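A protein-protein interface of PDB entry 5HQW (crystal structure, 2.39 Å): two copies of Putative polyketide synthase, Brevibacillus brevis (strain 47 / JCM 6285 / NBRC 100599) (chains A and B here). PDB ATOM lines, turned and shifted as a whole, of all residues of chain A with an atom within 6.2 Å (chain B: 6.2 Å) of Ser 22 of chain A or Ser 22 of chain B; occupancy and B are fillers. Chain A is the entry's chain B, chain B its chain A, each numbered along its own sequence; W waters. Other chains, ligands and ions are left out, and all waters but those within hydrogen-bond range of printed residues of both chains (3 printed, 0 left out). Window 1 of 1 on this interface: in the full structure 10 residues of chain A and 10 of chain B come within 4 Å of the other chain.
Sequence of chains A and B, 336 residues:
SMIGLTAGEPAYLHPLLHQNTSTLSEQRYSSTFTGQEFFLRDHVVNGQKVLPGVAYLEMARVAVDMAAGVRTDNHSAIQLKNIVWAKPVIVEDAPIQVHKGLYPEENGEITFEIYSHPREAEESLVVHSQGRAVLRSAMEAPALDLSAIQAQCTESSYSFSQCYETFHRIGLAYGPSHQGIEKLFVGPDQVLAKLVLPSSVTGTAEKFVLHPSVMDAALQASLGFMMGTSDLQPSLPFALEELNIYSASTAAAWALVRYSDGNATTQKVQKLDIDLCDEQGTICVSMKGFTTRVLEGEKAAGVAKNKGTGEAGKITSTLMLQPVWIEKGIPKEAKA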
ATOM      1  N   ASN A  20     -23.539  19.689   0.818  1.00  0.00           N
ATOM      2  CA  ASN A  20     -23.635  20.610  -0.307  1.00  0.00           C
ATOM      3  C   ASN A  20     -23.049  19.934  -1.541  1.00  0.00           C
ATOM      4  O   ASN A  20     -21.854  19.620  -1.572  1.00  0.00           O
ATOM      5  CB  ASN A  20     -22.896  21.911   0.002  1.00  0.00           C
ATOM      6  CG  ASN A  20     -23.024  22.942  -1.108  1.00  0.00           C
ATOM      7  OD1 ASN A  20     -23.348  22.612  -2.250  1.00  0.00           O
ATOM      8  ND2 ASN A  20     -22.758  24.199  -0.775  1.00  0.00           N
ATOM      9  N   THR A  21     -23.890  19.700  -2.549  1.00  0.00           N
ATOM     10  CA  THR A  21     -23.485  19.017  -3.773  1.00  0.00           C
ATOM     11  C   THR A  21     -23.647  19.910  -4.999  1.00  0.00           C
ATOM     12  O   THR A  21     -23.936  19.426  -6.095  1.00  0.00           O
ATOM     13  CB  THR A  21     -24.283  17.726  -3.950  1.00  0.00           C
ATOM     14  OG1 THR A  21     -25.684  18.022  -3.900  1.00  0.00           O
ATOM     15  CG2 THR A  21     -23.934  16.723  -2.862  1.00  0.00           C
ATOM     16  N   SER A  22     -23.460  21.215  -4.828  1.00  0.00           N
ATOM     17  CA  SER A  22     -23.726  22.160  -5.903  1.00  0.00           C
ATOM     18  C   SER A  22     -22.694  22.033  -7.018  1.00  0.00           C
ATOM     19  O   SER A  22     -21.506  21.808  -6.771  1.00  0.00           O
ATOM     20  CB  SER A  22     -23.732  23.587  -5.361  1.00  0.00           C
ATOM     21  OG  SER A  22     -24.824  23.792  -4.485  1.00  0.00           O
ATOM     22  N   THR A  23     -23.160  22.182  -8.252  1.00  0.00           N
ATOM     23  CA  THR A  23     -22.309  22.225  -9.432  1.00  0.00           C
ATOM     24  C   THR A  23     -22.433  23.597 -10.085  1.00  0.00           C
ATOM     25  O   THR A  23     -23.253  24.427  -9.686  1.00  0.00           O
ATOM     26  CB  THR A  23     -22.693  21.126 -10.430  1.00  0.00           C
ATOM     27  OG1 THR A  23     -23.979  21.418 -10.987  1.00  0.00           O
ATOM     28  CG2 THR A  23     -22.751  19.773  -9.739  1.00  0.00           C
ATOM     29  N   LEU A  24     -21.601  23.836 -11.101  1.00  0.00           N
ATOM     30  CA  LEU A  24     -21.714  25.083 -11.848  1.00  0.00           C
ATOM     31  C   LEU A  24     -23.103  25.239 -12.440  1.00  0.00           C
ATOM     32  O   LEU A  24     -23.609  26.361 -12.564  1.00  0.00           O
ATOM     33  CB  LEU A  24     -20.664  25.143 -12.959  1.00  0.00           C
ATOM     34  CG  LEU A  24     -19.195  25.225 -12.543  1.00  0.00           C
ATOM     35  CD1 LEU A  24     -18.312  25.220 -13.774  1.00  0.00           C
ATOM     36  CD2 LEU A  24     -18.924  26.451 -11.696  1.00  0.00           C
ATOM     37  N   GLU A  26     -25.968  23.829 -11.167  1.00  0.00           N
ATOM     38  CA  GLU A  26     -27.065  23.721 -10.215  1.00  0.00           C
ATOM     39  C   GLU A  26     -26.570  23.914  -8.790  1.00  0.00           C
ATOM     40  O   GLU A  26     -25.564  23.320  -8.389  1.00  0.00           O
ATOM     41  CB  GLU A  26     -27.750  22.356 -10.364  1.00  0.00           C
ATOM     42  CG  GLU A  26     -28.850  22.069  -9.359  1.00  0.00           C
ATOM     43  CD  GLU A  26     -29.386  20.657  -9.488  1.00  0.00           C
ATOM     44  OE1 GLU A  26     -28.940  19.936 -10.405  1.00  0.00           O
ATOM     45  OE2 GLU A  26     -30.249  20.270  -8.673  1.00  0.00           O
ATOM     46  N   GLN A  27     -27.285  24.744  -8.032  1.00  0.00           N
ATOM     47  CA  GLN A  27     -27.095  24.828  -6.590  1.00  0.00           C
ATOM     48  C   GLN A  27     -27.928  23.733  -5.938  1.00  0.00           C
ATOM     49  O   GLN A  27     -29.143  23.663  -6.154  1.00  0.00           O
ATOM     50  CB  GLN A  27     -27.516  26.205  -6.078  1.00  0.00           C
ATOM     51  CG  GLN A  27     -27.315  26.407  -4.581  1.00  0.00           C
ATOM     52  CD  GLN A  27     -25.865  26.666  -4.218  1.00  0.00           C
ATOM     53  OE1 GLN A  27     -25.033  26.926  -5.088  1.00  0.00           O
ATOM     54  NE2 GLN A  27     -25.557  26.598  -2.929  1.00  0.00           N
ATOM     55  N   ARG A  28     -27.292  22.880  -5.137  1.00  0.00           N
ATOM     56  CA  ARG A  28     -27.948  21.652  -4.717  1.00  0.00           C
ATOM     57  C   ARG A  28     -27.395  21.180  -3.382  1.00  0.00           C
ATOM     58  O   ARG A  28     -26.198  21.312  -3.110  1.00  0.00           O
ATOM     59  CB  ARG A  28     -27.770  20.557  -5.772  1.00  0.00           C
ATOM     60  CG  ARG A  28     -28.494  19.261  -5.458  1.00  0.00           C
ATOM     61  CD  ARG A  28     -28.232  18.229  -6.537  1.00  0.00           C
ATOM     62  NE  ARG A  28     -26.803  17.976  -6.705  1.00  0.00           N
ATOM     63  CZ  ARG A  28     -26.266  17.377  -7.762  1.00  0.00           C
ATOM     64  NH1 ARG A  28     -27.033  16.968  -8.763  1.00  0.00           N
ATOM     65  NH2 ARG A  28     -24.954  17.190  -7.819  1.00  0.00           N
ATOM     66  N   TYR A  29     -28.282  20.627  -2.557  1.00  0.00           N
ATOM     67  CA  TYR A  29     -27.904  19.990  -1.305  1.00  0.00           C
ATOM     68  C   TYR A  29     -28.516  18.599  -1.257  1.00  0.00           C
ATOM     69  O   TYR A  29     -29.623  18.370  -1.749  1.00  0.00           O
ATOM     70  CB  TYR A  29     -28.363  20.813  -0.095  1.00  0.00           C
ATOM     71  CG  TYR A  29     -27.791  22.209  -0.075  1.00  0.00           C
ATOM     72  CD1 TYR A  29     -26.573  22.472   0.535  1.00  0.00           C
ATOM     73  CD2 TYR A  29     -28.463  23.265  -0.678  1.00  0.00           C
ATOM     74  CE1 TYR A  29     -26.043  23.746   0.553  1.00  0.00           C
ATOM     75  CE2 TYR A  29     -27.942  24.542  -0.666  1.00  0.00           C
ATOM     76  CZ  TYR A  29     -26.731  24.778  -0.050  1.00  0.00           C
ATOM     77  OH  TYR A  29     -26.206  26.050  -0.037  1.00  0.00           O
ATOM     78  N   MET A  66     -28.151  29.029   3.690  1.00  0.00           N
ATOM     79  CA  MET A  66     -26.765  28.771   3.325  1.00  0.00           C
ATOM     80  C   MET A  66     -26.487  29.073   1.861  1.00  0.00           C
ATOM     81  O   MET A  66     -25.408  29.580   1.531  1.00  0.00           O
ATOM     82  CB  MET A  66     -26.403  27.319   3.633  1.00  0.00           C
ATOM     83  CG  MET A  66     -26.390  27.001   5.117  1.00  0.00           C
ATOM     84  SD  MET A  66     -25.651  25.397   5.459  1.00  0.00           S
ATOM     85  CE  MET A  66     -23.929  25.745   5.082  1.00  0.00           C
ATOM     86  N   ALA A  67     -27.438  28.783   0.970  1.00  0.00           N
ATOM     87  CA  ALA A  67     -27.207  29.025  -0.448  1.00  0.00           C
ATOM     88  C   ALA A  67     -27.067  30.514  -0.724  1.00  0.00           C
ATOM     89  O   ALA A  67     -26.242  30.922  -1.551  1.00  0.00           O
ATOM     90  CB  ALA A  67     -28.342  28.429  -1.274  1.00  0.00           C
ATOM     91  N   ASN B  20     -17.402  21.083  -0.250  1.00  0.00           N
ATOM     92  CA  ASN B  20     -18.097  21.945  -1.200  1.00  0.00           C
ATOM     93  C   ASN B  20     -18.873  22.995  -0.409  1.00  0.00           C
ATOM     94  O   ASN B  20     -19.816  22.665   0.314  1.00  0.00           O
ATOM     95  CB  ASN B  20     -19.026  21.112  -2.079  1.00  0.00           C
ATOM     96  CG  ASN B  20     -19.738  21.936  -3.139  1.00  0.00           C
ATOM     97  OD1 ASN B  20     -19.841  23.159  -3.037  1.00  0.00           O
ATOM     98  ND2 ASN B  20     -20.250  21.259  -4.162  1.00  0.00           N
ATOM     99  N   THR B  21     -18.481  24.261  -0.554  1.00  0.00           N
ATOM    100  CA  THR B  21     -19.096  25.365   0.176  1.00  0.00           C
ATOM    101  C   THR B  21     -19.738  26.362  -0.781  1.00  0.00           C
ATOM    102  O   THR B  21     -19.767  27.564  -0.509  1.00  0.00           O
ATOM    103  CB  THR B  21     -18.071  26.072   1.062  1.00  0.00           C
ATOM    104  OG1 THR B  21     -16.969  26.516   0.260  1.00  0.00           O
ATOM    105  CG2 THR B  21     -17.557  25.135   2.143  1.00  0.00           C
ATOM    106  N   SER B  22     -20.264  25.871  -1.899  1.00  0.00           N
ATOM    107  CA  SER B  22     -20.751  26.752  -2.950  1.00  0.00           C
ATOM    108  C   SER B  22     -21.999  27.504  -2.507  1.00  0.00           C
ATOM    109  O   SER B  22     -22.862  26.962  -1.811  1.00  0.00           O
ATOM    110  CB  SER B  22     -21.055  25.949  -4.212  1.00  0.00           C
ATOM    111  OG  SER B  22     -19.871  25.411  -4.769  1.00  0.00           O
ATOM    112  N   THR B  23     -22.088  28.762  -2.926  1.00  0.00           N
ATOM    113  CA  THR B  23     -23.258  29.598  -2.714  1.00  0.00           C
ATOM    114  C   THR B  23     -23.874  29.941  -4.067  1.00  0.00           C
ATOM    115  O   THR B  23     -23.314  29.641  -5.125  1.00  0.00           O
ATOM    116  CB  THR B  23     -22.893  30.878  -1.951  1.00  0.00           C
ATOM    117  OG1 THR B  23     -22.071  31.712  -2.776  1.00  0.00           O
ATOM    118  CG2 THR B  23     -22.140  30.540  -0.666  1.00  0.00           C
ATOM    119  N   LEU B  24     -25.047  30.576  -4.026  1.00  0.00           N
ATOM    120  CA  LEU B  24     -25.694  31.002  -5.264  1.00  0.00           C
ATOM    121  C   LEU B  24     -24.808  31.960  -6.045  1.00  0.00           C
ATOM    122  O   LEU B  24     -24.800  31.946  -7.281  1.00  0.00           O
ATOM    123  CB  LEU B  24     -27.036  31.665  -4.955  1.00  0.00           C
ATOM    124  CG  LEU B  24     -28.108  30.775  -4.332  1.00  0.00           C
ATOM    125  CD1 LEU B  24     -29.349  31.592  -4.034  1.00  0.00           C
ATOM    126  CD2 LEU B  24     -28.451  29.620  -5.262  1.00  0.00           C
ATOM    127  N   GLU B  26     -21.408  32.108  -5.829  1.00  0.00           N
ATOM    128  CA  GLU B  26     -20.064  31.607  -6.083  1.00  0.00           C
ATOM    129  C   GLU B  26     -20.013  30.094  -5.937  1.00  0.00           C
ATOM    130  O   GLU B  26     -20.519  29.541  -4.956  1.00  0.00           O
ATOM    131  CB  GLU B  26     -19.060  32.252  -5.121  1.00  0.00           C
ATOM    132  CG  GLU B  26     -17.639  31.717  -5.243  1.00  0.00           C
ATOM    133  CD  GLU B  26     -16.718  32.275  -4.177  1.00  0.00           C
ATOM    134  OE1 GLU B  26     -17.175  33.131  -3.388  1.00  0.00           O
ATOM    135  OE2 GLU B  26     -15.544  31.853  -4.123  1.00  0.00           O
ATOM    136  N   GLN B  27     -19.391  29.438  -6.914  1.00  0.00           N
ATOM    137  CA  GLN B  27     -19.025  28.032  -6.797  1.00  0.00           C
ATOM    138  C   GLN B  27     -17.694  27.957  -6.064  1.00  0.00           C
ATOM    139  O   GLN B  27     -16.714  28.579  -6.491  1.00  0.00           O
ATOM    140  CB  GLN B  27     -18.931  27.387  -8.177  1.00  0.00           C
ATOM    141  CG  GLN B  27     -18.567  25.911  -8.155  1.00  0.00           C
ATOM    142  CD  GLN B  27     -19.727  25.030  -7.752  1.00  0.00           C
ATOM    143  OE1 GLN B  27     -20.875  25.473  -7.707  1.00  0.00           O
ATOM    144  NE2 GLN B  27     -19.434  23.769  -7.454  1.00  0.00           N
ATOM    145  N   ARG B  28     -17.653  27.202  -4.969  1.00  0.00           N
ATOM    146  CA  ARG B  28     -16.537  27.292  -4.037  1.00  0.00           C
ATOM    147  C   ARG B  28     -16.347  25.971  -3.307  1.00  0.00           C
ATOM    148  O   ARG B  28     -17.317  25.287  -2.975  1.00  0.00           O
ATOM    149  CB  ARG B  28     -16.766  28.417  -3.022  1.00  0.00           C
ATOM    150  CG  ARG B  28     -15.630  28.616  -2.023  1.00  0.00           C
ATOM    151  CD  ARG B  28     -15.948  29.740  -1.041  1.00  0.00           C
ATOM    152  NE  ARG B  28     -17.205  29.509  -0.333  1.00  0.00           N
ATOM    153  CZ  ARG B  28     -17.881  30.445   0.327  1.00  0.00           C
ATOM    154  NH1 ARG B  28     -17.432  31.694   0.376  1.00  0.00           N
ATOM    155  NH2 ARG B  28     -19.017  30.132   0.936  1.00  0.00           N
ATOM    156  N   TYR B  29     -15.084  25.630  -3.064  1.00  0.00           N
ATOM    157  CA  TYR B  29     -14.707  24.490  -2.247  1.00  0.00           C
ATOM    158  C   TYR B  29     -13.720  24.966  -1.191  1.00  0.00           C
ATOM    159  O   TYR B  29     -12.922  25.877  -1.437  1.00  0.00           O
ATOM    160  CB  TYR B  29     -14.097  23.368  -3.095  1.00  0.00           C
ATOM    161  CG  TYR B  29     -15.022  22.868  -4.183  1.00  0.00           C
ATOM    162  CD1 TYR B  29     -15.915  21.833  -3.943  1.00  0.00           C
ATOM    163  CD2 TYR B  29     -15.008  23.439  -5.449  1.00  0.00           C
ATOM    164  CE1 TYR B  29     -16.764  21.377  -4.932  1.00  0.00           C
ATOM    165  CE2 TYR B  29     -15.854  22.989  -6.446  1.00  0.00           C
ATOM    166  CZ  TYR B  29     -16.728  21.958  -6.182  1.00  0.00           C
ATOM    167  OH  TYR B  29     -17.571  21.509  -7.171  1.00  0.00           O
ATOM    168  N   MET B  66     -15.148  18.319 -10.342  1.00  0.00           N
ATOM    169  CA  MET B  66     -16.371  18.150  -9.569  1.00  0.00           C
ATOM    170  C   MET B  66     -17.385  19.244  -9.872  1.00  0.00           C
ATOM    171  O   MET B  66     -18.591  18.979  -9.922  1.00  0.00           O
ATOM    172  CB  MET B  66     -16.050  18.147  -8.076  1.00  0.00           C
ATOM    173  CG  MET B  66     -15.203  16.972  -7.633  1.00  0.00           C
ATOM    174  SD  MET B  66     -15.154  16.823  -5.845  1.00  0.00           S
ATOM    175  CE  MET B  66     -16.832  16.272  -5.544  1.00  0.00           C
ATOM    176  N   ALA B  67     -16.918  20.480 -10.061  1.00  0.00           N
ATOM    177  CA  ALA B  67     -17.834  21.580 -10.340  1.00  0.00           C
ATOM    178  C   ALA B  67     -18.484  21.413 -11.706  1.00  0.00           C
ATOM    179  O   ALA B  67     -19.668  21.727 -11.880  1.00  0.00           O
ATOM    180  CB  ALA B  67     -17.096  22.910 -10.242  1.00  0.00           C
HETATM  181  O   HOH W   1     -23.864  26.988   0.762  1.00  0.00           O
HETATM  182  O   HOH W   2     -19.525  19.748  -7.205  1.00  0.00           O
HETATM  183  O   HOH W   3     -20.740  20.086   2.208  1.00  0.00           O
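The backbone carbonyl oxygen (O) of Asn 20 of chain A lies close to the side-chain amide nitrogen (ND2) of Asn 20 of chain B.
O of Ser 22 of chain A lies within hydrogen-bond range of ND2 of Asn 20 of chain B (2.9 Å).
O of Ser 22 of chain B lies within hydrogen-bond range of ND2 of Asn 20 of chain A, 3.0 Å away.
The backbone carbonyl oxygen (O) of Ser 22 of chain B is in hydrogen-bond range of the side-chain amide nitrogen (NE2) of Gln 27 of chain A.
The side-chain amide oxygen (OE1) of Gln 27 of chain A sits close to the backbone carbonyl oxygen (O) of Thr 23 of chain B (3.2 Å).
The backbone NH of Leu 24 of chain B lies within hydrogen-bond range of the backbone carbonyl oxygen of Ala 67 of chain A, 2.8 Å away.
The backbone carbonyl oxygen of Ser 22 of chain A lies within hydrogen-bond range of the side-chain amide nitrogen of Gln 27 of chain B (2.9 Å).
OE1 of Gln 27 of chain B lies close to O of Thr 23 of chain A, at 3.3 Å.
O of Ala 67 of chain B lies within hydrogen-bond range of N of Leu 24 of chain A (3.0 Å).
The side-chain hydroxyl (OG) of Ser 22 of chain B lies within hydrogen-bond range of the side-chain amide oxygen (OD1) of Asn 20 of chain B.
The side-chain hydroxyl (OG1) of Thr 23 of chain B lies within hydrogen-bond range of the backbone NH (N) of Glu 26 of chain B (3.1 Å).
OH of Tyr 29 of chain B sits at hydrogen-bond distance from N of Ala 67 of chain B (3.1 Å).
The backbone NH (N) of Thr 21 of chain A sits at hydrogen-bond distance from the backbone carbonyl oxygen (O) of Arg 28 of chain A, 2.9 Å away.
The backbone NH of Glu 26 of chain A lies within hydrogen-bond range of the side-chain hydroxyl of Thr 23 of chain A (3.1 Å).
The side-chain amide nitrogen (NE2) of Gln 27 of chain A lies within hydrogen-bond range of the side-chain hydroxyl (OH) of Tyr 29 of chain A, at 3.0 Å.
Among the printed residues, merely in contact across the chains: Asn 20 of chain A with Thr 21 of chain B (3.7 Å), Thr 21 of chain A with Asn 20 of chain B (3.7 Å), Ser 22 of chain A with Ser 22 of chain B (3.8 Å), Ser 22 of chain A with Tyr 29 of chain B (3.97 Å), Thr 23 of chain A with Ala 67 of chain B (3.4 Å), Leu 24 of chain A with Gln 27 of chain B (3.6 Å), Gln 27 of chain A with Leu 24 of chain B (3.5 Å), Tyr 29 of chain A with Ser 22 of chain B (3.9 Å) and Ala 67 of chain A with Thr 23 of chain B (3.4 Å).
Ser 22 of chain A touches four residues of chain B.
Printed residues of chain B within 4 Å of Tyr 29 of chain A: Ser 22.
Met 66 of chain A touches none of the printed residues of chain B.
Of the printed residues of chain B, Ala 67 of chain A touches Thr 23 (3.4 Å) and Leu 24 (2.8 Å).
Of the printed residues of chain A, Ser 22 of chain B touches Asn 20 (3.0 Å), Ser 22 (3.8 Å), Gln 27 (2.9 Å) and Tyr 29 (3.9 Å).
Arg 28 of chain B touches none of the printed residues of chain A.
Of the printed residues of chain A, Tyr 29 of chain B touches Ser 22 (3.97 Å).
Of the printed residues of chain A, Ala 67 of chain B touches Thr 23 and Leu 24.
The nearest residue of chain A that does not touch Ser 22 of chain B is Met 66 of chain A (5.0 Å).
The nearest printed residue of chain B that does not touch Tyr 29 of chain A is Thr 23 of chain B (5.3 Å).
Of the 11 printed residues of chain A, 8 touch a printed residue of chain B.
Hydrophobic or aromatic side chains of chain A that line the printed part of chain B: Leu 24, Tyr 29 and Ala 67.
Of the 11 printed residues of chain B, 8 touch a printed residue of chain A.
Printed residues of chain B that touch a printed residue of chain A: Asn 20, Thr 21, Ser 22, Thr 23, Leu 24, Gln 27, Tyr 29 and Ala 67.
Hydrophobic or aromatic side chains of chain B that line the printed part of chain A: Leu 24, Tyr 29 and Ala 67.
Among the printed residues, no Asp or Glu carboxylate lies within 4 Å of a Lys or Arg side-chain nitrogen of the other chain.
Asn 20 of chain A touches Thr 21 of chain B, and with the chains exchanged Thr 21 of chain A touches Asn 20 of chain B.
Asn 20 of chain A touches Ser 22 of chain B, and with the chains exchanged Ser 22 of chain A touches Asn 20 of chain B.
Thr 23 of chain A touches Gln 27 of chain B, and with the chains exchanged Gln 27 of chain A touches Thr 23 of chain B.
Thr 23 of chain A touches Ala 67 of chain B, and with the chains exchanged Ala 67 of chain A touches Thr 23 of chain B.
Of the 18 pairs that touch across the chains among the printed residues, 18 have their exchanged pair printed and touching as well.
Water W2 lies within hydrogen-bond range of OH of Tyr 29 of chain B, O of Ser 22 of chain A, O of Met 66 of chain B and ND2 of Asn 20 of chain B.
Water W1 lies within hydrogen-bond range of the side-chain hydroxyl (OH) of Tyr 29 of chain A, the backbone carbonyl oxygen (O) of Ser 22 of chain B, the backbone carbonyl oxygen (O) of Met 66 of chain A and the side-chain amide nitrogen (ND2) of Asn 20 of chain A.
Water W3 lies within hydrogen-bond range of the backbone NH of Asn 20 of chain A (3.2 Å) and the backbone carbonyl oxygen of Asn 20 of chain B (3.3 Å).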
